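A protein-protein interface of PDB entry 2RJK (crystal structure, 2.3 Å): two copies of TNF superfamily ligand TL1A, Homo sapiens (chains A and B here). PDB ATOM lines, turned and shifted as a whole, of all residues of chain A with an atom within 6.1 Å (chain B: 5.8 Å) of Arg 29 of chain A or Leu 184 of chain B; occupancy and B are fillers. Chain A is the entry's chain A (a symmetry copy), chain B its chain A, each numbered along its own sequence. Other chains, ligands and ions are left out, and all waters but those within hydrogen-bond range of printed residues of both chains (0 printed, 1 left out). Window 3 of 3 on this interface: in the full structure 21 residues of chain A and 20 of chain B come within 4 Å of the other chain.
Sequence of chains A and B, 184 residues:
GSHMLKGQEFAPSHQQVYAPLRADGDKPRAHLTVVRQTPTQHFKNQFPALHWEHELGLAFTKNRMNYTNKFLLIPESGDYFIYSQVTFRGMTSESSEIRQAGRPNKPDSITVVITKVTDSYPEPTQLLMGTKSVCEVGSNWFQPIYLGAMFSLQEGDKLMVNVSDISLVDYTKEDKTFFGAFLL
Among the printed residues, merely in contact across the chains: Arg 29 of chain A with Met 150 of chain B (3.7 Å), Ala 30 of chain A with Met 150 of chain B (3.2 Å), His 31 of chain A with Met 150 of chain B (3.6 Å), Phe 60 of chain A with Met 150 of chain B (3.7 Å), Ala 181 of chain A with Met 150 of chain B (3.7 Å), Phe 182 of chain A with Phe 81 of chain B (3.6 Å), Phe 182 of chain A with Met 150 of chain B (3.95 Å) and Phe 182 of chain A with Leu 184 of chain B (3.6 Å).
The side-chain carboxylate of Asp 79 of chain B lies within salt-bridge range of the side-chain amino group of Lys 62 of chain A, at 2.9 Å. OD2 of Asp 79 of chain B lies within salt-bridge range of NH1 of Arg 29 of chain A, at 2.8 Å. O of Leu 184 of chain B is in salt-bridge range of NH2 of Arg 29 of chain A.
Arg 29 of chain A touches just these residues of chain B: Asp 79 (2.8 Å), Met 150 (3.7 Å) and Leu 184 (3.8 Å). Of the printed residues of chain B, Ala 181 of chain A touches Met 150 (3.7 Å). Of the printed residues of chain A, Phe 81 of chain B touches Phe 182 (3.6 Å). Printed residues of chain B within 4 Å of Phe 182 of chain A: Phe 81 (3.6 Å), Met 150 (3.95 Å) and Leu 184 (3.6 Å). Of the printed residues of chain B, Ala 30 of chain A touches Met 150. Leu 184 of chain A touches none of the printed residues of chain B. The nearest printed residue of chain B that does not touch Arg 29 of chain A is Lys 27 of chain B (6.3 Å). The nearest residue of chain A that does not touch Leu 184 of chain B is Leu 184 of chain A (5.1 Å).
NZ of Lys 27 of chain B is in salt-bridge range of OXT of Leu 184 of chain B (3.0 Å). O of Arg 29 of chain A is in hydrogen-bond range of N of Lys 62 of chain A (3.0 Å). N of Phe 182 of chain B is in hydrogen-bond range of O of Phe 81 of chain B, 2.9 Å away. O of Ala 30 of chain A lies within hydrogen-bond range of N of Ala 181 of chain A (3.0 Å). The backbone NH of Leu 184 of chain B sits at hydrogen-bond distance from the backbone carbonyl oxygen of Asp 79 of chain B (2.9 Å). The backbone carbonyl oxygen (O) of His 31 of chain A sits at hydrogen-bond distance from the backbone NH (N) of Phe 60 of chain A, at 2.8 Å.
Phe 182 of chain A touches Leu 184 of chain B, but with the chains exchanged Leu 184 of chain A does not touch Phe 182 of chain B (6.7 Å). Of the 11 pairs that touch across the chains among the printed residues, none has its exchanged pair printed and touching as well.
Of the 8 printed residues of chain B, 4 touch a printed residue of chain A. Of the 17 printed residues of chain A, 7 touch a printed residue of chain B. Among the printed residues, Asp or Glu carboxylates within 4 Å of a Lys or Arg side-chain nitrogen of the other chain: Arg 29 of chain A with Asp 79 of chain B (2.8 Å) and Lys 62 of chain A with Asp 79 of chain B (2.9 Å).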
ATOM      1  N   GLY A  25       5.207  28.328  20.293  1.00  0.00           N
ATOM      2  CA  GLY A  25       5.267  28.172  18.802  1.00  0.00           C
ATOM      3  C   GLY A  25       4.281  27.112  18.319  1.00  0.00           C
ATOM      4  O   GLY A  25       3.166  26.988  18.861  1.00  0.00           O
ATOM      5  N   ASP A  26       4.678  26.342  17.305  1.00  0.00           N
ATOM      6  CA  ASP A  26       3.884  25.182  16.910  1.00  0.00           C
ATOM      7  C   ASP A  26       4.314  23.915  17.692  1.00  0.00           C
ATOM      8  O   ASP A  26       5.099  23.084  17.218  1.00  0.00           O
ATOM      9  CB  ASP A  26       3.943  24.962  15.398  1.00  0.00           C
ATOM     10  CG  ASP A  26       5.355  24.763  14.896  1.00  0.00           C
ATOM     11  OD1 ASP A  26       5.516  24.335  13.727  1.00  0.00           O
ATOM     12  OD2 ASP A  26       6.298  25.035  15.681  1.00  0.00           O
ATOM     13  N   LYS A  27       3.817  23.784  18.915  1.00  0.00           N
ATOM     14  CA  LYS A  27       4.148  22.618  19.699  1.00  0.00           C
ATOM     15  C   LYS A  27       3.028  21.633  19.551  1.00  0.00           C
ATOM     16  O   LYS A  27       1.869  22.017  19.514  1.00  0.00           O
ATOM     17  CB  LYS A  27       4.379  23.013  21.129  1.00  0.00           C
ATOM     18  CG  LYS A  27       5.665  23.803  21.211  1.00  0.00           C
ATOM     19  CD  LYS A  27       5.933  24.272  22.571  1.00  0.00           C
ATOM     20  CE  LYS A  27       7.377  24.693  22.654  1.00  0.00           C
ATOM     21  NZ  LYS A  27       7.616  25.328  23.959  1.00  0.00           N
ATOM     22  N   PRO A  28       3.373  20.362  19.355  1.00  0.00           N
ATOM     23  CA  PRO A  28       2.285  19.374  19.307  1.00  0.00           C
ATOM     24  C   PRO A  28       1.422  19.447  20.573  1.00  0.00           C
ATOM     25  O   PRO A  28       1.955  19.538  21.710  1.00  0.00           O
ATOM     26  CB  PRO A  28       3.025  18.038  19.214  1.00  0.00           C
ATOM     27  CG  PRO A  28       4.423  18.416  18.625  1.00  0.00           C
ATOM     28  CD  PRO A  28       4.714  19.780  19.185  1.00  0.00           C
ATOM     29  N   ARG A  29       0.106  19.414  20.374  1.00  0.00           N
ATOM     30  CA  ARG A  29      -0.835  19.477  21.464  1.00  0.00           C
ATOM     31  C   ARG A  29      -2.123  18.765  21.086  1.00  0.00           C
ATOM     32  O   ARG A  29      -2.559  18.848  19.973  1.00  0.00           O
ATOM     33  CB  ARG A  29      -1.232  20.924  21.726  1.00  0.00           C
ATOM     34  CG  ARG A  29      -0.161  21.793  22.242  1.00  0.00           C
ATOM     35  CD  ARG A  29      -0.628  23.291  22.307  1.00  0.00           C
ATOM     36  NE  ARG A  29       0.542  24.024  22.728  1.00  0.00           N
ATOM     37  CZ  ARG A  29       0.791  25.263  22.400  1.00  0.00           C
ATOM     38  NH1 ARG A  29      -0.069  25.943  21.668  1.00  0.00           N
ATOM     39  NH2 ARG A  29       1.899  25.805  22.818  1.00  0.00           N
ATOM     40  N   ALA A  30      -2.763  18.131  22.054  1.00  0.00           N
ATOM     41  CA  ALA A  30      -4.045  17.525  21.836  1.00  0.00           C
ATOM     42  C   ALA A  30      -4.817  17.484  23.162  1.00  0.00           C
ATOM     43  O   ALA A  30      -4.231  17.152  24.183  1.00  0.00           O
ATOM     44  CB  ALA A  30      -3.862  16.114  21.310  1.00  0.00           C
ATOM     45  N   HIS A  31      -6.122  17.779  23.099  1.00  0.00           N
ATOM     46  CA  HIS A  31      -7.075  17.484  24.133  1.00  0.00           C
ATOM     47  C   HIS A  31      -8.163  16.590  23.565  1.00  0.00           C
ATOM     48  O   HIS A  31      -8.878  17.012  22.690  1.00  0.00           O
ATOM     49  CB  HIS A  31      -7.712  18.788  24.683  1.00  0.00           C
ATOM     50  CG  HIS A  31      -8.643  18.576  25.842  1.00  0.00           C
ATOM     51  ND1 HIS A  31      -8.209  18.216  27.106  1.00  0.00           N
ATOM     52  CD2 HIS A  31      -9.994  18.710  25.934  1.00  0.00           C
ATOM     53  CE1 HIS A  31      -9.258  18.137  27.922  1.00  0.00           C
ATOM     54  NE2 HIS A  31     -10.348  18.437  27.235  1.00  0.00           N
ATOM     55  N   PHE A  60      -9.372  18.479  20.341  1.00  0.00           N
ATOM     56  CA  PHE A  60      -8.591  18.888  19.209  1.00  0.00           C
ATOM     57  C   PHE A  60      -7.245  18.210  19.205  1.00  0.00           C
ATOM     58  O   PHE A  60      -6.776  17.726  20.251  1.00  0.00           O
ATOM     59  CB  PHE A  60      -8.366  20.418  19.224  1.00  0.00           C
ATOM     60  CG  PHE A  60      -7.396  20.893  20.301  1.00  0.00           C
ATOM     61  CD1 PHE A  60      -6.025  20.954  20.053  1.00  0.00           C
ATOM     62  CD2 PHE A  60      -7.870  21.333  21.537  1.00  0.00           C
ATOM     63  CE1 PHE A  60      -5.091  21.425  21.024  1.00  0.00           C
ATOM     64  CE2 PHE A  60      -6.966  21.802  22.555  1.00  0.00           C
ATOM     65  CZ  PHE A  60      -5.558  21.849  22.291  1.00  0.00           C
ATOM     66  N   THR A  61      -6.609  18.226  18.031  1.00  0.00           N
ATOM     67  CA  THR A  61      -5.197  17.820  17.854  1.00  0.00           C
ATOM     68  C   THR A  61      -4.600  18.849  16.925  1.00  0.00           C
ATOM     69  O   THR A  61      -5.299  19.359  16.065  1.00  0.00           O
ATOM     70  CB  THR A  61      -5.045  16.402  17.198  1.00  0.00           C
ATOM     71  OG1 THR A  61      -5.695  16.381  15.927  1.00  0.00           O
ATOM     72  CG2 THR A  61      -5.715  15.302  18.051  1.00  0.00           C
ATOM     73  N   LYS A  62      -3.345  19.170  17.099  1.00  0.00           N
ATOM     74  CA  LYS A  62      -2.748  20.171  16.287  1.00  0.00           C
ATOM     75  C   LYS A  62      -1.276  20.064  16.337  1.00  0.00           C
ATOM     76  O   LYS A  62      -0.753  19.379  17.149  1.00  0.00           O
ATOM     77  CB  LYS A  62      -3.196  21.529  16.732  1.00  0.00           C
ATOM     78  CG  LYS A  62      -2.414  22.123  17.815  1.00  0.00           C
ATOM     79  CD  LYS A  62      -3.239  23.155  18.503  1.00  0.00           C
ATOM     80  CE  LYS A  62      -2.798  24.535  18.151  1.00  0.00           C
ATOM     81  NZ  LYS A  62      -3.764  25.540  18.564  1.00  0.00           N
ATOM     82  N   ASN A  63      -0.610  20.714  15.413  1.00  0.00           N
ATOM     83  CA  ASN A  63       0.816  20.605  15.267  1.00  0.00           C
ATOM     84  C   ASN A  63       1.449  19.253  15.195  1.00  0.00           C
ATOM     85  O   ASN A  63       2.423  19.013  15.834  1.00  0.00           O
ATOM     86  CB  ASN A  63       1.513  21.467  16.269  1.00  0.00           C
ATOM     87  CG  ASN A  63       1.027  22.837  16.232  1.00  0.00           C
ATOM     88  OD1 ASN A  63       0.756  23.361  15.189  1.00  0.00           O
ATOM     89  ND2 ASN A  63       0.894  23.434  17.357  1.00  0.00           N
ATOM     90  N   MET A  65       0.463  16.369  16.069  1.00  0.00           N
ATOM     91  CA  MET A  65      -0.157  15.446  16.978  1.00  0.00           C
ATOM     92  C   MET A  65      -1.218  14.721  16.211  1.00  0.00           C
ATOM     93  O   MET A  65      -1.991  15.327  15.539  1.00  0.00           O
ATOM     94  CB  MET A  65      -0.768  16.233  18.137  1.00  0.00           C
ATOM     95  CG  MET A  65      -1.008  15.478  19.404  1.00  0.00           C
ATOM     96  SD  MET A  65       0.414  14.712  20.118  1.00  0.00           S
ATOM     97  CE  MET A  65       0.799  15.804  21.410  1.00  0.00           C
ATOM     98  N   TYR A  80       6.950  16.004  27.476  1.00  0.00           N
ATOM     99  CA  TYR A  80       5.532  16.320  27.336  1.00  0.00           C
ATOM    100  C   TYR A  80       4.871  16.269  28.671  1.00  0.00           C
ATOM    101  O   TYR A  80       5.200  15.412  29.523  1.00  0.00           O
ATOM    102  CB  TYR A  80       4.822  15.261  26.466  1.00  0.00           C
ATOM    103  CG  TYR A  80       5.107  15.388  25.004  1.00  0.00           C
ATOM    104  CD1 TYR A  80       4.165  15.947  24.129  1.00  0.00           C
ATOM    105  CD2 TYR A  80       6.320  14.956  24.479  1.00  0.00           C
ATOM    106  CE1 TYR A  80       4.431  16.053  22.755  1.00  0.00           C
ATOM    107  CE2 TYR A  80       6.577  15.047  23.117  1.00  0.00           C
ATOM    108  CZ  TYR A  80       5.642  15.600  22.265  1.00  0.00           C
ATOM    109  OH  TYR A  80       5.930  15.713  20.928  1.00  0.00           O
ATOM    110  N   ALA A 181      -2.208  15.990  26.019  1.00  0.00           N
ATOM    111  CA  ALA A 181      -0.738  15.967  26.046  1.00  0.00           C
ATOM    112  C   ALA A 181      -0.225  17.160  25.290  1.00  0.00           C
ATOM    113  O   ALA A 181      -0.808  17.584  24.267  1.00  0.00           O
ATOM    114  CB  ALA A 181      -0.224  14.676  25.434  1.00  0.00           C
ATOM    115  N   PHE A 182       0.815  17.787  25.797  1.00  0.00           N
ATOM    116  CA  PHE A 182       1.411  18.888  25.027  1.00  0.00           C
ATOM    117  C   PHE A 182       2.911  18.873  25.211  1.00  0.00           C
ATOM    118  O   PHE A 182       3.404  18.570  26.324  1.00  0.00           O
ATOM    119  CB  PHE A 182       0.886  20.264  25.418  1.00  0.00           C
ATOM    120  CG  PHE A 182       0.790  20.533  26.921  1.00  0.00           C
ATOM    121  CD1 PHE A 182       1.787  21.282  27.582  1.00  0.00           C
ATOM    122  CD2 PHE A 182      -0.352  20.115  27.652  1.00  0.00           C
ATOM    123  CE1 PHE A 182       1.682  21.573  29.027  1.00  0.00           C
ATOM    124  CE2 PHE A 182      -0.525  20.437  29.067  1.00  0.00           C
ATOM    125  CZ  PHE A 182       0.530  21.147  29.753  1.00  0.00           C
ATOM    126  N   LEU A 183       3.639  19.150  24.131  1.00  0.00           N
ATOM    127  CA  LEU A 183       5.087  19.346  24.247  1.00  0.00           C
ATOM    128  C   LEU A 183       5.377  20.592  25.107  1.00  0.00           C
ATOM    129  O   LEU A 183       4.856  21.688  24.864  1.00  0.00           O
ATOM    130  CB  LEU A 183       5.712  19.572  22.857  1.00  0.00           C
ATOM    131  CG  LEU A 183       7.239  19.735  22.798  1.00  0.00           C
ATOM    132  CD1 LEU A 183       7.929  18.376  23.158  1.00  0.00           C
ATOM    133  CD2 LEU A 183       7.709  20.189  21.394  1.00  0.00           C
ATOM    134  N   LEU A 184       6.237  20.450  26.093  1.00  0.00           N
ATOM    135  CA  LEU A 184       6.521  21.574  26.969  1.00  0.00           C
ATOM    136  C   LEU A 184       7.349  22.652  26.260  1.00  0.00           C
ATOM    137  O   LEU A 184       8.255  22.351  25.471  1.00  0.00           O
ATOM    138  CB  LEU A 184       7.261  21.078  28.219  1.00  0.00           C
ATOM    139  CG  LEU A 184       6.377  20.189  29.091  1.00  0.00           C
ATOM    140  CD1 LEU A 184       7.191  19.747  30.270  1.00  0.00           C
ATOM    141  CD2 LEU A 184       5.174  20.991  29.566  1.00  0.00           C
ATOM    142  OXT LEU A 184       7.144  23.854  26.472  1.00  0.00           O
ATOM    143  N   LYS B  27       4.196  35.428  29.289  1.00  0.00           N
ATOM    144  CA  LYS B  27       2.974  34.718  28.994  1.00  0.00           C
ATOM    145  C   LYS B  27       1.993  35.021  30.085  1.00  0.00           C
ATOM    146  O   LYS B  27       2.367  35.108  31.246  1.00  0.00           O
ATOM    147  CB  LYS B  27       3.256  33.248  28.869  1.00  0.00           C
ATOM    148  CG  LYS B  27       4.050  33.014  27.604  1.00  0.00           C
ATOM    149  CD  LYS B  27       4.412  31.606  27.437  1.00  0.00           C
ATOM    150  CE  LYS B  27       4.839  31.389  26.010  1.00  0.00           C
ATOM    151  NZ  LYS B  27       5.369  30.025  25.872  1.00  0.00           N
ATOM    152  N   ASP B  79      -3.572  28.592  23.467  1.00  0.00           N
ATOM    153  CA  ASP B  79      -3.853  27.395  24.240  1.00  0.00           C
ATOM    154  C   ASP B  79      -3.337  27.553  25.663  1.00  0.00           C
ATOM    155  O   ASP B  79      -2.175  27.869  25.870  1.00  0.00           O
ATOM    156  CB  ASP B  79      -3.174  26.208  23.579  1.00  0.00           C
ATOM    157  CG  ASP B  79      -3.645  26.020  22.154  1.00  0.00           C
ATOM    158  OD1 ASP B  79      -4.874  26.151  21.924  1.00  0.00           O
ATOM    159  OD2 ASP B  79      -2.788  25.774  21.276  1.00  0.00           O
ATOM    160  N   TYR B  80      -4.212  27.311  26.632  1.00  0.00           N
ATOM    161  CA  TYR B  80      -3.901  27.525  28.042  1.00  0.00           C
ATOM    162  C   TYR B  80      -4.065  26.248  28.793  1.00  0.00           C
ATOM    163  O   TYR B  80      -4.984  25.445  28.510  1.00  0.00           O
ATOM    164  CB  TYR B  80      -4.893  28.524  28.674  1.00  0.00           C
ATOM    165  CG  TYR B  80      -4.647  29.947  28.290  1.00  0.00           C
ATOM    166  CD1 TYR B  80      -4.029  30.839  29.178  1.00  0.00           C
ATOM    167  CD2 TYR B  80      -5.023  30.418  27.037  1.00  0.00           C
ATOM    168  CE1 TYR B  80      -3.811  32.178  28.820  1.00  0.00           C
ATOM    169  CE2 TYR B  80      -4.821  31.748  26.688  1.00  0.00           C
ATOM    170  CZ  TYR B  80      -4.211  32.616  27.571  1.00  0.00           C
ATOM    171  OH  TYR B  80      -3.988  33.917  27.193  1.00  0.00           O
ATOM    172  N   PHE B  81      -3.238  26.086  29.812  1.00  0.00           N
ATOM    173  CA  PHE B  81      -3.509  25.035  30.760  1.00  0.00           C
ATOM    174  C   PHE B  81      -4.203  25.694  31.927  1.00  0.00           C
ATOM    175  O   PHE B  81      -3.824  26.775  32.392  1.00  0.00           O
ATOM    176  CB  PHE B  81      -2.258  24.341  31.202  1.00  0.00           C
ATOM    177  CG  PHE B  81      -2.517  23.114  32.053  1.00  0.00           C
ATOM    178  CD1 PHE B  81      -2.815  21.904  31.454  1.00  0.00           C
ATOM    179  CD2 PHE B  81      -2.459  23.185  33.456  1.00  0.00           C
ATOM    180  CE1 PHE B  81      -3.041  20.736  32.226  1.00  0.00           C
ATOM    181  CE2 PHE B  81      -2.702  22.011  34.265  1.00  0.00           C
ATOM    182  CZ  PHE B  81      -2.967  20.795  33.628  1.00  0.00           C
ATOM    183  N   MET B 150      -5.867  21.374  29.074  1.00  0.00           N
ATOM    184  CA  MET B 150      -5.505  22.387  28.092  1.00  0.00           C
ATOM    185  C   MET B 150      -6.702  22.734  27.186  1.00  0.00           C
ATOM    186  O   MET B 150      -7.417  21.839  26.726  1.00  0.00           O
ATOM    187  CB  MET B 150      -4.323  21.911  27.279  1.00  0.00           C
ATOM    188  CG  MET B 150      -4.086  22.664  25.958  1.00  0.00           C
ATOM    189  SD  MET B 150      -2.752  21.839  25.027  1.00  0.00           S
ATOM    190  CE  MET B 150      -3.450  20.171  24.861  1.00  0.00           C
ATOM    191  N   PHE B 182      -2.363  29.269  32.664  1.00  0.00           N
ATOM    192  CA  PHE B 182      -1.197  29.906  32.033  1.00  0.00           C
ATOM    193  C   PHE B 182      -1.212  29.619  30.550  1.00  0.00           C
ATOM    194  O   PHE B 182      -1.598  28.502  30.130  1.00  0.00           O
ATOM    195  CB  PHE B 182       0.138  29.445  32.606  1.00  0.00           C
ATOM    196  CG  PHE B 182       0.284  27.936  32.810  1.00  0.00           C
ATOM    197  CD1 PHE B 182       0.989  27.150  31.872  1.00  0.00           C
ATOM    198  CD2 PHE B 182      -0.202  27.322  33.992  1.00  0.00           C
ATOM    199  CE1 PHE B 182       1.161  25.697  32.082  1.00  0.00           C
ATOM    200  CE2 PHE B 182       0.004  25.901  34.268  1.00  0.00           C
ATOM    201  CZ  PHE B 182       0.667  25.090  33.274  1.00  0.00           C
ATOM    202  N   LEU B 183      -0.842  30.621  29.754  1.00  0.00           N
ATOM    203  CA  LEU B 183      -0.641  30.388  28.320  1.00  0.00           C
ATOM    204  C   LEU B 183       0.535  29.414  28.109  1.00  0.00           C
ATOM    205  O   LEU B 183       1.641  29.605  28.630  1.00  0.00           O
ATOM    206  CB  LEU B 183      -0.299  31.709  27.604  1.00  0.00           C
ATOM    207  CG  LEU B 183      -0.116  31.648  26.080  1.00  0.00           C
ATOM    208  CD1 LEU B 183      -1.493  31.349  25.395  1.00  0.00           C
ATOM    209  CD2 LEU B 183       0.454  32.975  25.521  1.00  0.00           C
ATOM    210  N   LEU B 184       0.323  28.385  27.318  1.00  0.00           N
ATOM    211  CA  LEU B 184       1.377  27.405  27.112  1.00  0.00           C
ATOM    212  C   LEU B 184       2.516  27.967  26.254  1.00  0.00           C
ATOM    213  O   LEU B 184       2.288  28.711  25.291  1.00  0.00           O
ATOM    214  CB  LEU B 184       0.790  26.149  26.453  1.00  0.00           C
ATOM    215  CG  LEU B 184      -0.175  25.414  27.381  1.00  0.00           C
ATOM    216  CD1 LEU B 184      -0.702  24.220  26.644  1.00  0.00           C
ATOM    217  CD2 LEU B 184       0.573  24.963  28.626  1.00  0.00           C
ATOM    218  OXT LEU B 184       3.695  27.675  26.492  1.00  0.00           O
